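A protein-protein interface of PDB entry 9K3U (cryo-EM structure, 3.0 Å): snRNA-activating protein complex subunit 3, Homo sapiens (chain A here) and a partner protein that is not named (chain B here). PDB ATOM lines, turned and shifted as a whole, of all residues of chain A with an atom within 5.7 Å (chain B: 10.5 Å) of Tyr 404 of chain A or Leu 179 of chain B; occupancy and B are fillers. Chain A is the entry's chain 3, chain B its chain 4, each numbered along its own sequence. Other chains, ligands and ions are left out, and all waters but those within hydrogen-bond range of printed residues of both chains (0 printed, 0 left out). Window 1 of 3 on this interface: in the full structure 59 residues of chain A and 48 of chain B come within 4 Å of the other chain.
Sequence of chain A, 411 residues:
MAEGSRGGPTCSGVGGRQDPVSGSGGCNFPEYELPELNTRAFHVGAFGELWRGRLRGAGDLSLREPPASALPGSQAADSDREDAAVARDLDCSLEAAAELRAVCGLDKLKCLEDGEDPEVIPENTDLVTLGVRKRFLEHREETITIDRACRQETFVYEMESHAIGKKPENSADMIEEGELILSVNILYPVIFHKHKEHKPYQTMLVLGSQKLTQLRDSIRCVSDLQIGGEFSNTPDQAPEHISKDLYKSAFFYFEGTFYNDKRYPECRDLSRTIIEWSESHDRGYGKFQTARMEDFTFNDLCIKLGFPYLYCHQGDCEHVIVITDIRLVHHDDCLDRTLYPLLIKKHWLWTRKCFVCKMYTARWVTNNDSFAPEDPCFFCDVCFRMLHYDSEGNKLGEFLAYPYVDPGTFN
The backbone carbonyl oxygen (O) of Arg 363 of chain A is in hydrogen-bond range of the backbone NH (N) of Tyr 404 of chain A (2.8 Å). The side-chain carboxylate of Asp 406 of chain A sits at hydrogen-bond distance from the backbone NH of Arg 352 of chain A (2.7 Å). The side-chain hydroxyl (OH) of Tyr 404 of chain A lies within hydrogen-bond range of the side-chain carboxylate (OD1) of Asp 406 of chain A, at 3.2 Å. O of Val 405 of chain A sits close to OE1 of Gln 226 of chain A, 2.8 Å away. O of Arg 352 of chain A sits at hydrogen-bond distance from N of Ala 362 of chain A, at 2.8 Å. The backbone NH of Tyr 402 of chain A lies within hydrogen-bond range of the backbone carbonyl oxygen of Val 365 of chain A, at 2.8 Å.
Gln 226 of chain A touches Ile 173 of chain B. Gln 226 of chain A touches Ala 175 of chain B (CD to CB, 3.2 Å). Arg 352 of chain A touches Val 181 of chain B. NE of Arg 363 of chain A touches OH of Tyr 377 of chain B, at 3.7 Å. Pro 376 of chain A touches Leu 179 of chain B (CB to O, 3.4 Å). Phe 378 of chain A touches Leu 179 of chain B. Tyr 402 of chain A touches Gly 172 of chain B. Leu 179 of chain B touches Tyr 404 of chain A (CD2 to CE1, 3.3 Å).
No residue of chain B comes within 4 Å of Ala 362 of chain A. No residue of chain B comes within 4 Å of Val 365 of chain A. Pro 376 of chain A touches just one residue of chain B: Leu 179 (3.4 Å). Printed residues of chain B within 4 Å of Phe 378 of chain A: Leu 179. No residue of chain B comes within 4 Å of Pro 403 of chain A. No residue of chain B comes within 4 Å of Asp 406 of chain A. Printed residues of chain A within 4 Å of Ile 173 of chain B: Gln 226. Of chain A, only Pro 376 (3.4 Å), Phe 378 (3.3 Å) and Tyr 404 (3.3 Å) come within 4 Å of Leu 179 of chain B. Leu 180 of chain B touches none of the printed residues of chain A.
Of the 16 printed residues of chain B, 6 touch a printed residue of chain A. Printed residues of chain B that touch a printed residue of chain A: Gly 172, Ile 173, Ala 175, Leu 179, Val 181 and Tyr 377. Hydrophobic or aromatic side chains of chain A that line the printed part of chain B: Pro 376, Phe 378, Tyr 402 and Tyr 404. Among the printed residues, 8 pairs touch across the chains. Among the printed residues, no Asp or Glu carboxylate lies within 4 Å of a Lys or Arg side-chain nitrogen of the other chain.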
ATOM      1  N   GLN A 226     -17.008  -1.604   7.437  1.00  0.00           N
ATOM      2  CA  GLN A 226     -16.081  -2.700   7.681  1.00  0.00           C
ATOM      3  C   GLN A 226     -14.714  -2.167   8.094  1.00  0.00           C
ATOM      4  O   GLN A 226     -14.270  -1.110   7.639  1.00  0.00           O
ATOM      5  CB  GLN A 226     -15.942  -3.567   6.428  1.00  0.00           C
ATOM      6  CG  GLN A 226     -17.152  -4.446   6.138  1.00  0.00           C
ATOM      7  CD  GLN A 226     -17.405  -5.517   7.192  1.00  0.00           C
ATOM      8  OE1 GLN A 226     -18.512  -6.045   7.290  1.00  0.00           O
ATOM      9  NE2 GLN A 226     -16.382  -5.848   7.980  1.00  0.00           N
ATOM     10  N   ARG A 352     -26.190 -11.591  12.040  1.00  0.00           N
ATOM     11  CA  ARG A 352     -25.546 -12.834  12.452  1.00  0.00           C
ATOM     12  C   ARG A 352     -25.461 -12.861  13.972  1.00  0.00           C
ATOM     13  O   ARG A 352     -24.819 -11.995  14.578  1.00  0.00           O
ATOM     14  CB  ARG A 352     -24.156 -12.955  11.825  1.00  0.00           C
ATOM     15  CG  ARG A 352     -23.438 -14.262  12.134  1.00  0.00           C
ATOM     16  CD  ARG A 352     -24.144 -15.457  11.509  1.00  0.00           C
ATOM     17  NE  ARG A 352     -23.444 -16.711  11.778  1.00  0.00           N
ATOM     18  CZ  ARG A 352     -23.815 -17.893  11.295  1.00  0.00           C
ATOM     19  NH1 ARG A 352     -24.883 -17.994  10.515  1.00  0.00           N
ATOM     20  NH2 ARG A 352     -23.116 -18.979  11.596  1.00  0.00           N
ATOM     21  N   ALA A 362     -23.539 -10.999  16.841  1.00  0.00           N
ATOM     22  CA  ALA A 362     -22.093 -11.172  16.849  1.00  0.00           C
ATOM     23  C   ALA A 362     -21.387  -9.865  16.508  1.00  0.00           C
ATOM     24  O   ALA A 362     -21.890  -9.039  15.742  1.00  0.00           O
ATOM     25  CB  ALA A 362     -21.681 -12.258  15.854  1.00  0.00           C
ATOM     26  N   ARG A 363     -20.201  -9.687  17.095  1.00  0.00           N
ATOM     27  CA  ARG A 363     -19.371  -8.519  16.834  1.00  0.00           C
ATOM     28  C   ARG A 363     -17.925  -8.863  16.509  1.00  0.00           C
ATOM     29  O   ARG A 363     -17.182  -7.970  16.084  1.00  0.00           O
ATOM     30  CB  ARG A 363     -19.389  -7.565  18.037  1.00  0.00           C
ATOM     31  CG  ARG A 363     -20.772  -7.030  18.381  1.00  0.00           C
ATOM     32  CD  ARG A 363     -20.721  -6.069  19.559  1.00  0.00           C
ATOM     33  NE  ARG A 363     -19.897  -4.898  19.275  1.00  0.00           N
ATOM     34  CZ  ARG A 363     -19.674  -3.910  20.139  1.00  0.00           C
ATOM     35  NH1 ARG A 363     -20.210  -3.946  21.350  1.00  0.00           N
ATOM     36  NH2 ARG A 363     -18.908  -2.887  19.789  1.00  0.00           N
ATOM     37  N   TRP A 364     -17.501 -10.113  16.692  1.00  0.00           N
ATOM     38  CA  TRP A 364     -16.141 -10.541  16.407  1.00  0.00           C
ATOM     39  C   TRP A 364     -16.172 -11.848  15.630  1.00  0.00           C
ATOM     40  O   TRP A 364     -16.996 -12.726  15.905  1.00  0.00           O
ATOM     41  CB  TRP A 364     -15.333 -10.725  17.696  1.00  0.00           C
ATOM     42  CG  TRP A 364     -15.002  -9.440  18.385  1.00  0.00           C
ATOM     43  CD1 TRP A 364     -15.813  -8.718  19.212  1.00  0.00           C
ATOM     44  CD2 TRP A 364     -13.762  -8.723  18.315  1.00  0.00           C
ATOM     45  NE1 TRP A 364     -15.157  -7.596  19.657  1.00  0.00           N
ATOM     46  CE2 TRP A 364     -13.897  -7.575  19.121  1.00  0.00           C
ATOM     47  CE3 TRP A 364     -12.552  -8.939  17.646  1.00  0.00           C
ATOM     48  CZ2 TRP A 364     -12.869  -6.648  19.278  1.00  0.00           C
ATOM     49  CZ3 TRP A 364     -11.535  -8.015  17.803  1.00  0.00           C
ATOM     50  CH2 TRP A 364     -11.700  -6.886  18.612  1.00  0.00           C
ATOM     51  N   VAL A 365     -15.270 -11.969  14.658  1.00  0.00           N
ATOM     52  CA  VAL A 365     -15.115 -13.176  13.858  1.00  0.00           C
ATOM     53  C   VAL A 365     -13.744 -13.763  14.158  1.00  0.00           C
ATOM     54  O   VAL A 365     -12.736 -13.047  14.123  1.00  0.00           O
ATOM     55  CB  VAL A 365     -15.275 -12.895  12.351  1.00  0.00           C
ATOM     56  CG1 VAL A 365     -14.254 -11.865  11.876  1.00  0.00           C
ATOM     57  CG2 VAL A 365     -15.156 -14.188  11.553  1.00  0.00           C
ATOM     58  N   PRO A 376     -15.361 -20.682  10.480  1.00  0.00           N
ATOM     59  CA  PRO A 376     -15.947 -19.352  10.312  1.00  0.00           C
ATOM     60  C   PRO A 376     -16.839 -19.126  11.534  1.00  0.00           C
ATOM     61  O   PRO A 376     -18.039 -19.275  11.414  1.00  0.00           O
ATOM     62  CB  PRO A 376     -16.793 -19.447   9.034  1.00  0.00           C
ATOM     63  CG  PRO A 376     -16.441 -20.793   8.432  1.00  0.00           C
ATOM     64  CD  PRO A 376     -16.021 -21.653   9.605  1.00  0.00           C
ATOM     65  N   PHE A 378     -18.299 -16.988  15.182  1.00  0.00           N
ATOM     66  CA  PHE A 378     -18.815 -15.624  15.474  1.00  0.00           C
ATOM     67  C   PHE A 378     -19.127 -15.498  16.966  1.00  0.00           C
ATOM     68  O   PHE A 378     -19.838 -16.366  17.504  1.00  0.00           O
ATOM     69  CB  PHE A 378     -20.066 -15.338  14.643  1.00  0.00           C
ATOM     70  CG  PHE A 378     -19.854 -15.464  13.157  1.00  0.00           C
ATOM     71  CD1 PHE A 378     -19.240 -14.450  12.445  1.00  0.00           C
ATOM     72  CD2 PHE A 378     -20.248 -16.606  12.483  1.00  0.00           C
ATOM     73  CE1 PHE A 378     -19.037 -14.573  11.079  1.00  0.00           C
ATOM     74  CE2 PHE A 378     -20.045 -16.728  11.117  1.00  0.00           C
ATOM     75  CZ  PHE A 378     -19.442 -15.709  10.420  1.00  0.00           C
ATOM     76  N   TYR A 402     -10.986 -10.817  14.415  1.00  0.00           N
ATOM     77  CA  TYR A 402     -11.171  -9.592  13.659  1.00  0.00           C
ATOM     78  C   TYR A 402     -12.506  -8.963  14.018  1.00  0.00           C
ATOM     79  O   TYR A 402     -13.456  -9.675  14.361  1.00  0.00           O
ATOM     80  CB  TYR A 402     -11.123  -9.858  12.146  1.00  0.00           C
ATOM     81  CG  TYR A 402      -9.868 -10.563  11.683  1.00  0.00           C
ATOM     82  CD1 TYR A 402      -9.791 -11.949  11.675  1.00  0.00           C
ATOM     83  CD2 TYR A 402      -8.761  -9.845  11.251  1.00  0.00           C
ATOM     84  CE1 TYR A 402      -8.648 -12.601  11.252  1.00  0.00           C
ATOM     85  CE2 TYR A 402      -7.614 -10.485  10.827  1.00  0.00           C
ATOM     86  CZ  TYR A 402      -7.562 -11.864  10.828  1.00  0.00           C
ATOM     87  OH  TYR A 402      -6.422 -12.508  10.408  1.00  0.00           O
ATOM     88  N   PRO A 403     -12.615  -7.628  13.952  1.00  0.00           N
ATOM     89  CA  PRO A 403     -13.913  -6.993  14.220  1.00  0.00           C
ATOM     90  C   PRO A 403     -14.946  -7.335  13.160  1.00  0.00           C
ATOM     91  O   PRO A 403     -14.818  -6.920  12.003  1.00  0.00           O
ATOM     92  CB  PRO A 403     -13.585  -5.494  14.223  1.00  0.00           C
ATOM     93  CG  PRO A 403     -12.111  -5.411  14.425  1.00  0.00           C
ATOM     94  CD  PRO A 403     -11.546  -6.631  13.775  1.00  0.00           C
ATOM     95  N   TYR A 404     -15.971  -8.091  13.541  1.00  0.00           N
ATOM     96  CA  TYR A 404     -17.018  -8.510  12.609  1.00  0.00           C
ATOM     97  C   TYR A 404     -18.096  -7.437  12.571  1.00  0.00           C
ATOM     98  O   TYR A 404     -18.941  -7.352  13.466  1.00  0.00           O
ATOM     99  CB  TYR A 404     -17.595  -9.859  13.022  1.00  0.00           C
ATOM    100  CG  TYR A 404     -18.791 -10.288  12.202  1.00  0.00           C
ATOM    101  CD1 TYR A 404     -18.629 -10.901  10.967  1.00  0.00           C
ATOM    102  CD2 TYR A 404     -20.084 -10.082  12.665  1.00  0.00           C
ATOM    103  CE1 TYR A 404     -19.720 -11.294  10.216  1.00  0.00           C
ATOM    104  CE2 TYR A 404     -21.182 -10.470  11.920  1.00  0.00           C
ATOM    105  CZ  TYR A 404     -20.993 -11.078  10.698  1.00  0.00           C
ATOM    106  OH  TYR A 404     -22.082 -11.467   9.952  1.00  0.00           O
ATOM    107  N   VAL A 405     -18.068  -6.609  11.529  1.00  0.00           N
ATOM    108  CA  VAL A 405     -19.086  -5.579  11.322  1.00  0.00           C
ATOM    109  C   VAL A 405     -20.270  -6.256  10.637  1.00  0.00           C
ATOM    110  O   VAL A 405     -20.244  -6.507   9.430  1.00  0.00           O
ATOM    111  CB  VAL A 405     -18.553  -4.403  10.500  1.00  0.00           C
ATOM    112  CG1 VAL A 405     -19.636  -3.353  10.311  1.00  0.00           C
ATOM    113  CG2 VAL A 405     -17.325  -3.800  11.172  1.00  0.00           C
ATOM    114  N   ASP A 406     -21.310  -6.558  11.405  1.00  0.00           N
ATOM    115  CA  ASP A 406     -22.449  -7.281  10.861  1.00  0.00           C
ATOM    116  C   ASP A 406     -23.135  -6.444   9.781  1.00  0.00           C
ATOM    117  O   ASP A 406     -23.232  -5.218   9.913  1.00  0.00           O
ATOM    118  CB  ASP A 406     -23.444  -7.623  11.968  1.00  0.00           C
ATOM    119  CG  ASP A 406     -24.604  -8.459  11.467  1.00  0.00           C
ATOM    120  OD1 ASP A 406     -24.419  -9.678  11.275  1.00  0.00           O
ATOM    121  OD2 ASP A 406     -25.699  -7.897  11.266  1.00  0.00           O
ATOM    122  N   PRO A 407     -23.617  -7.066   8.701  1.00  0.00           N
ATOM    123  CA  PRO A 407     -24.288  -6.280   7.653  1.00  0.00           C
ATOM    124  C   PRO A 407     -25.482  -5.487   8.156  1.00  0.00           C
ATOM    125  O   PRO A 407     -25.807  -4.442   7.580  1.00  0.00           O
ATOM    126  CB  PRO A 407     -24.710  -7.344   6.631  1.00  0.00           C
ATOM    127  CG  PRO A 407     -23.786  -8.484   6.857  1.00  0.00           C
ATOM    128  CD  PRO A 407     -23.501  -8.488   8.329  1.00  0.00           C
ATOM    129  N   GLY B 172      -6.563  -7.803   5.438  1.00  0.00           N
ATOM    130  CA  GLY B 172      -7.257  -8.749   6.288  1.00  0.00           C
ATOM    131  C   GLY B 172      -8.710  -8.386   6.512  1.00  0.00           C
ATOM    132  O   GLY B 172      -9.350  -8.901   7.434  1.00  0.00           O
ATOM    133  N   ILE B 173      -9.244  -7.494   5.678  1.00  0.00           N
ATOM    134  CA  ILE B 173     -10.630  -7.045   5.800  1.00  0.00           C
ATOM    135  C   ILE B 173     -11.507  -8.068   5.079  1.00  0.00           C
ATOM    136  O   ILE B 173     -11.708  -7.992   3.867  1.00  0.00           O
ATOM    137  CB  ILE B 173     -10.831  -5.629   5.253  1.00  0.00           C
ATOM    138  CG1 ILE B 173     -12.324  -5.313   5.129  1.00  0.00           C
ATOM    139  CG2 ILE B 173     -10.124  -5.449   3.906  1.00  0.00           C
ATOM    140  CD1 ILE B 173     -12.629  -3.839   4.964  1.00  0.00           C
ATOM    141  N   LYS B 174     -12.033  -9.029   5.833  1.00  0.00           N
ATOM    142  CA  LYS B 174     -12.917 -10.075   5.318  1.00  0.00           C
ATOM    143  C   LYS B 174     -14.314  -9.775   5.853  1.00  0.00           C
ATOM    144  O   LYS B 174     -14.712 -10.277   6.906  1.00  0.00           O
ATOM    145  CB  LYS B 174     -12.426 -11.455   5.745  1.00  0.00           C
ATOM    146  CG  LYS B 174     -10.980 -11.740   5.354  1.00  0.00           C
ATOM    147  CD  LYS B 174     -10.524 -13.121   5.804  1.00  0.00           C
ATOM    148  CE  LYS B 174     -10.478 -13.242   7.322  1.00  0.00           C
ATOM    149  NZ  LYS B 174      -9.947 -14.561   7.759  1.00  0.00           N
ATOM    150  N   ALA B 175     -15.060  -8.950   5.120  1.00  0.00           N
ATOM    151  CA  ALA B 175     -16.299  -8.390   5.650  1.00  0.00           C
ATOM    152  C   ALA B 175     -17.338  -9.456   5.967  1.00  0.00           C
ATOM    153  O   ALA B 175     -17.642  -9.697   7.140  1.00  0.00           O
ATOM    154  CB  ALA B 175     -16.881  -7.389   4.651  1.00  0.00           C
ATOM    155  N   PHE B 176     -17.897 -10.099   4.936  1.00  0.00           N
ATOM    156  CA  PHE B 176     -18.860 -11.171   5.161  1.00  0.00           C
ATOM    157  C   PHE B 176     -18.790 -12.275   4.112  1.00  0.00           C
ATOM    158  O   PHE B 176     -19.655 -13.161   4.114  1.00  0.00           O
ATOM    159  CB  PHE B 176     -20.285 -10.604   5.213  1.00  0.00           C
ATOM    160  CG  PHE B 176     -20.681  -9.840   3.984  1.00  0.00           C
ATOM    161  CD1 PHE B 176     -20.407  -8.489   3.875  1.00  0.00           C
ATOM    162  CD2 PHE B 176     -21.330 -10.474   2.937  1.00  0.00           C
ATOM    163  CE1 PHE B 176     -20.769  -7.782   2.749  1.00  0.00           C
ATOM    164  CE2 PHE B 176     -21.696  -9.772   1.806  1.00  0.00           C
ATOM    165  CZ  PHE B 176     -21.416  -8.424   1.711  1.00  0.00           C
ATOM    166  N   GLU B 177     -17.804 -12.263   3.217  1.00  0.00           N
ATOM    167  CA  GLU B 177     -17.810 -13.162   2.068  1.00  0.00           C
ATOM    168  C   GLU B 177     -17.324 -14.562   2.435  1.00  0.00           C
ATOM    169  O   GLU B 177     -18.075 -15.536   2.325  1.00  0.00           O
ATOM    170  CB  GLU B 177     -16.953 -12.579   0.940  1.00  0.00           C
ATOM    171  CG  GLU B 177     -17.713 -12.342  -0.355  1.00  0.00           C
ATOM    172  CD  GLU B 177     -18.818 -11.313  -0.204  1.00  0.00           C
ATOM    173  OE1 GLU B 177     -18.927 -10.709   0.884  1.00  0.00           O
ATOM    174  OE2 GLU B 177     -19.580 -11.113  -1.174  1.00  0.00           O
ATOM    175  N   GLU B 178     -16.071 -14.674   2.880  1.00  0.00           N
ATOM    176  CA  GLU B 178     -15.501 -15.992   3.140  1.00  0.00           C
ATOM    177  C   GLU B 178     -15.982 -16.568   4.466  1.00  0.00           C
ATOM    178  O   GLU B 178     -15.844 -17.774   4.699  1.00  0.00           O
ATOM    179  CB  GLU B 178     -13.971 -15.932   3.111  1.00  0.00           C
ATOM    180  CG  GLU B 178     -13.359 -14.681   3.729  1.00  0.00           C
ATOM    181  CD  GLU B 178     -13.149 -13.572   2.712  1.00  0.00           C
ATOM    182  OE1 GLU B 178     -12.702 -13.873   1.585  1.00  0.00           O
ATOM    183  OE2 GLU B 178     -13.438 -12.401   3.035  1.00  0.00           O
ATOM    184  N   LEU B 179     -16.540 -15.737   5.345  1.00  0.00           N
ATOM    185  CA  LEU B 179     -17.033 -16.216   6.630  1.00  0.00           C
ATOM    186  C   LEU B 179     -18.424 -16.832   6.548  1.00  0.00           C
ATOM    187  O   LEU B 179     -18.971 -17.225   7.584  1.00  0.00           O
ATOM    188  CB  LEU B 179     -17.029 -15.075   7.657  1.00  0.00           C
ATOM    189  CG  LEU B 179     -17.750 -13.769   7.308  1.00  0.00           C
ATOM    190  CD1 LEU B 179     -19.265 -13.945   7.281  1.00  0.00           C
ATOM    191  CD2 LEU B 179     -17.354 -12.682   8.297  1.00  0.00           C
ATOM    192  N   LEU B 180     -19.008 -16.927   5.353  1.00  0.00           N
ATOM    193  CA  LEU B 180     -20.313 -17.555   5.214  1.00  0.00           C
ATOM    194  C   LEU B 180     -20.221 -19.044   5.519  1.00  0.00           C
ATOM    195  O   LEU B 180     -19.171 -19.671   5.334  1.00  0.00           O
ATOM    196  CB  LEU B 180     -20.857 -17.343   3.801  1.00  0.00           C
ATOM    197  CG  LEU B 180     -21.123 -15.894   3.387  1.00  0.00           C
ATOM    198  CD1 LEU B 180     -21.538 -15.825   1.924  1.00  0.00           C
ATOM    199  CD2 LEU B 180     -22.184 -15.261   4.275  1.00  0.00           C
ATOM    200  N   VAL B 181     -21.325 -19.614   5.994  1.00  0.00           N
ATOM    201  CA  VAL B 181     -21.406 -21.028   6.335  1.00  0.00           C
ATOM    202  C   VAL B 181     -22.645 -21.619   5.676  1.00  0.00           C
ATOM    203  O   VAL B 181     -23.725 -21.018   5.711  1.00  0.00           O
ATOM    204  CB  VAL B 181     -21.441 -21.245   7.864  1.00  0.00           C
ATOM    205  CG1 VAL B 181     -22.684 -20.606   8.475  1.00  0.00           C
ATOM    206  CG2 VAL B 181     -21.373 -22.730   8.194  1.00  0.00           C
ATOM    207  N   THR B 182     -22.484 -22.793   5.074  1.00  0.00           N
ATOM    208  CA  THR B 182     -23.573 -23.510   4.426  1.00  0.00           C
ATOM    209  C   THR B 182     -23.869 -24.793   5.189  1.00  0.00           C
ATOM    210  O   THR B 182     -22.949 -25.484   5.637  1.00  0.00           O
ATOM    211  CB  THR B 182     -23.231 -23.838   2.970  1.00  0.00           C
ATOM    212  OG1 THR B 182     -22.042 -24.637   2.923  1.00  0.00           O
ATOM    213  CG2 THR B 182     -23.011 -22.561   2.169  1.00  0.00           C
ATOM    214  N   LYS B 183     -25.156 -25.104   5.339  1.00  0.00           N
ATOM    215  CA  LYS B 183     -25.557 -26.297   6.069  1.00  0.00           C
ATOM    216  C   LYS B 183     -24.983 -27.546   5.410  1.00  0.00           C
ATOM    217  O   LYS B 183     -24.891 -27.634   4.183  1.00  0.00           O
ATOM    218  CB  LYS B 183     -27.083 -26.390   6.134  1.00  0.00           C
ATOM    219  CG  LYS B 183     -27.741 -25.207   6.827  1.00  0.00           C
ATOM    220  CD  LYS B 183     -29.240 -25.412   6.966  1.00  0.00           C
ATOM    221  CE  LYS B 183     -29.920 -24.178   7.536  1.00  0.00           C
ATOM    222  NZ  LYS B 183     -31.399 -24.341   7.615  1.00  0.00           N
ATOM    223  N   ARG B 275     -15.688 -27.215   0.522  1.00  0.00           N
ATOM    224  CA  ARG B 275     -15.602 -27.205   1.977  1.00  0.00           C
ATOM    225  C   ARG B 275     -14.166 -26.922   2.393  1.00  0.00           C
ATOM    226  O   ARG B 275     -13.234 -27.576   1.911  1.00  0.00           O
ATOM    227  CB  ARG B 275     -16.071 -28.541   2.561  1.00  0.00           C
ATOM    228  CG  ARG B 275     -17.549 -28.834   2.341  1.00  0.00           C
ATOM    229  CD  ARG B 275     -18.435 -27.861   3.106  1.00  0.00           C
ATOM    230  NE  ARG B 275     -19.854 -28.173   2.962  1.00  0.00           N
ATOM    231  CZ  ARG B 275     -20.834 -27.487   3.540  1.00  0.00           C
ATOM    232  NH1 ARG B 275     -20.557 -26.442   4.311  1.00  0.00           N
ATOM    233  NH2 ARG B 275     -22.096 -27.845   3.349  1.00  0.00           N
ATOM    234  N   SER B 276     -13.993 -25.950   3.283  1.00  0.00           N
ATOM    235  CA  SER B 276     -12.660 -25.567   3.721  1.00  0.00           C
ATOM    236  C   SER B 276     -12.031 -26.671   4.567  1.00  0.00           C
ATOM    237  O   SER B 276     -12.715 -27.485   5.196  1.00  0.00           O
ATOM    238  CB  SER B 276     -12.715 -24.262   4.519  1.00  0.00           C
ATOM    239  OG  SER B 276     -13.529 -24.402   5.668  1.00  0.00           O
ATOM    240  N   GLU B 279     -12.988 -26.256   8.240  1.00  0.00           N
ATOM    241  CA  GLU B 279     -14.365 -26.677   8.463  1.00  0.00           C
ATOM    242  C   GLU B 279     -14.477 -28.193   8.459  1.00  0.00           C
ATOM    243  O   GLU B 279     -15.188 -28.773   9.290  1.00  0.00           O
ATOM    244  CB  GLU B 279     -15.278 -26.068   7.398  1.00  0.00           C
ATOM    245  CG  GLU B 279     -16.756 -26.364   7.606  1.00  0.00           C
ATOM    246  CD  GLU B 279     -17.630 -25.742   6.535  1.00  0.00           C
ATOM    247  OE1 GLU B 279     -17.080 -25.092   5.619  1.00  0.00           O
ATOM    248  OE2 GLU B 279     -18.866 -25.901   6.608  1.00  0.00           O
ATOM    249  N   TYR B 377     -29.359  -5.830  20.346  1.00  0.00           N
ATOM    250  CA  TYR B 377     -27.948  -5.705  19.997  1.00  0.00           C
ATOM    251  C   TYR B 377     -27.243  -4.696  20.895  1.00  0.00           C
ATOM    252  O   TYR B 377     -26.155  -4.972  21.416  1.00  0.00           O
ATOM    253  CB  TYR B 377     -27.802  -5.305  18.529  1.00  0.00           C
ATOM    254  CG  TYR B 377     -26.411  -4.837  18.165  1.00  0.00           C
ATOM    255  CD1 TYR B 377     -25.307  -5.653  18.369  1.00  0.00           C
ATOM    256  CD2 TYR B 377     -26.202  -3.582  17.613  1.00  0.00           C
ATOM    257  CE1 TYR B 377     -24.033  -5.231  18.039  1.00  0.00           C
ATOM    258  CE2 TYR B 377     -24.932  -3.149  17.278  1.00  0.00           C
ATOM    259  CZ  TYR B 377     -23.851  -3.979  17.492  1.00  0.00           C
ATOM    260  OH  TYR B 377     -22.585  -3.556  17.162  1.00  0.00           O
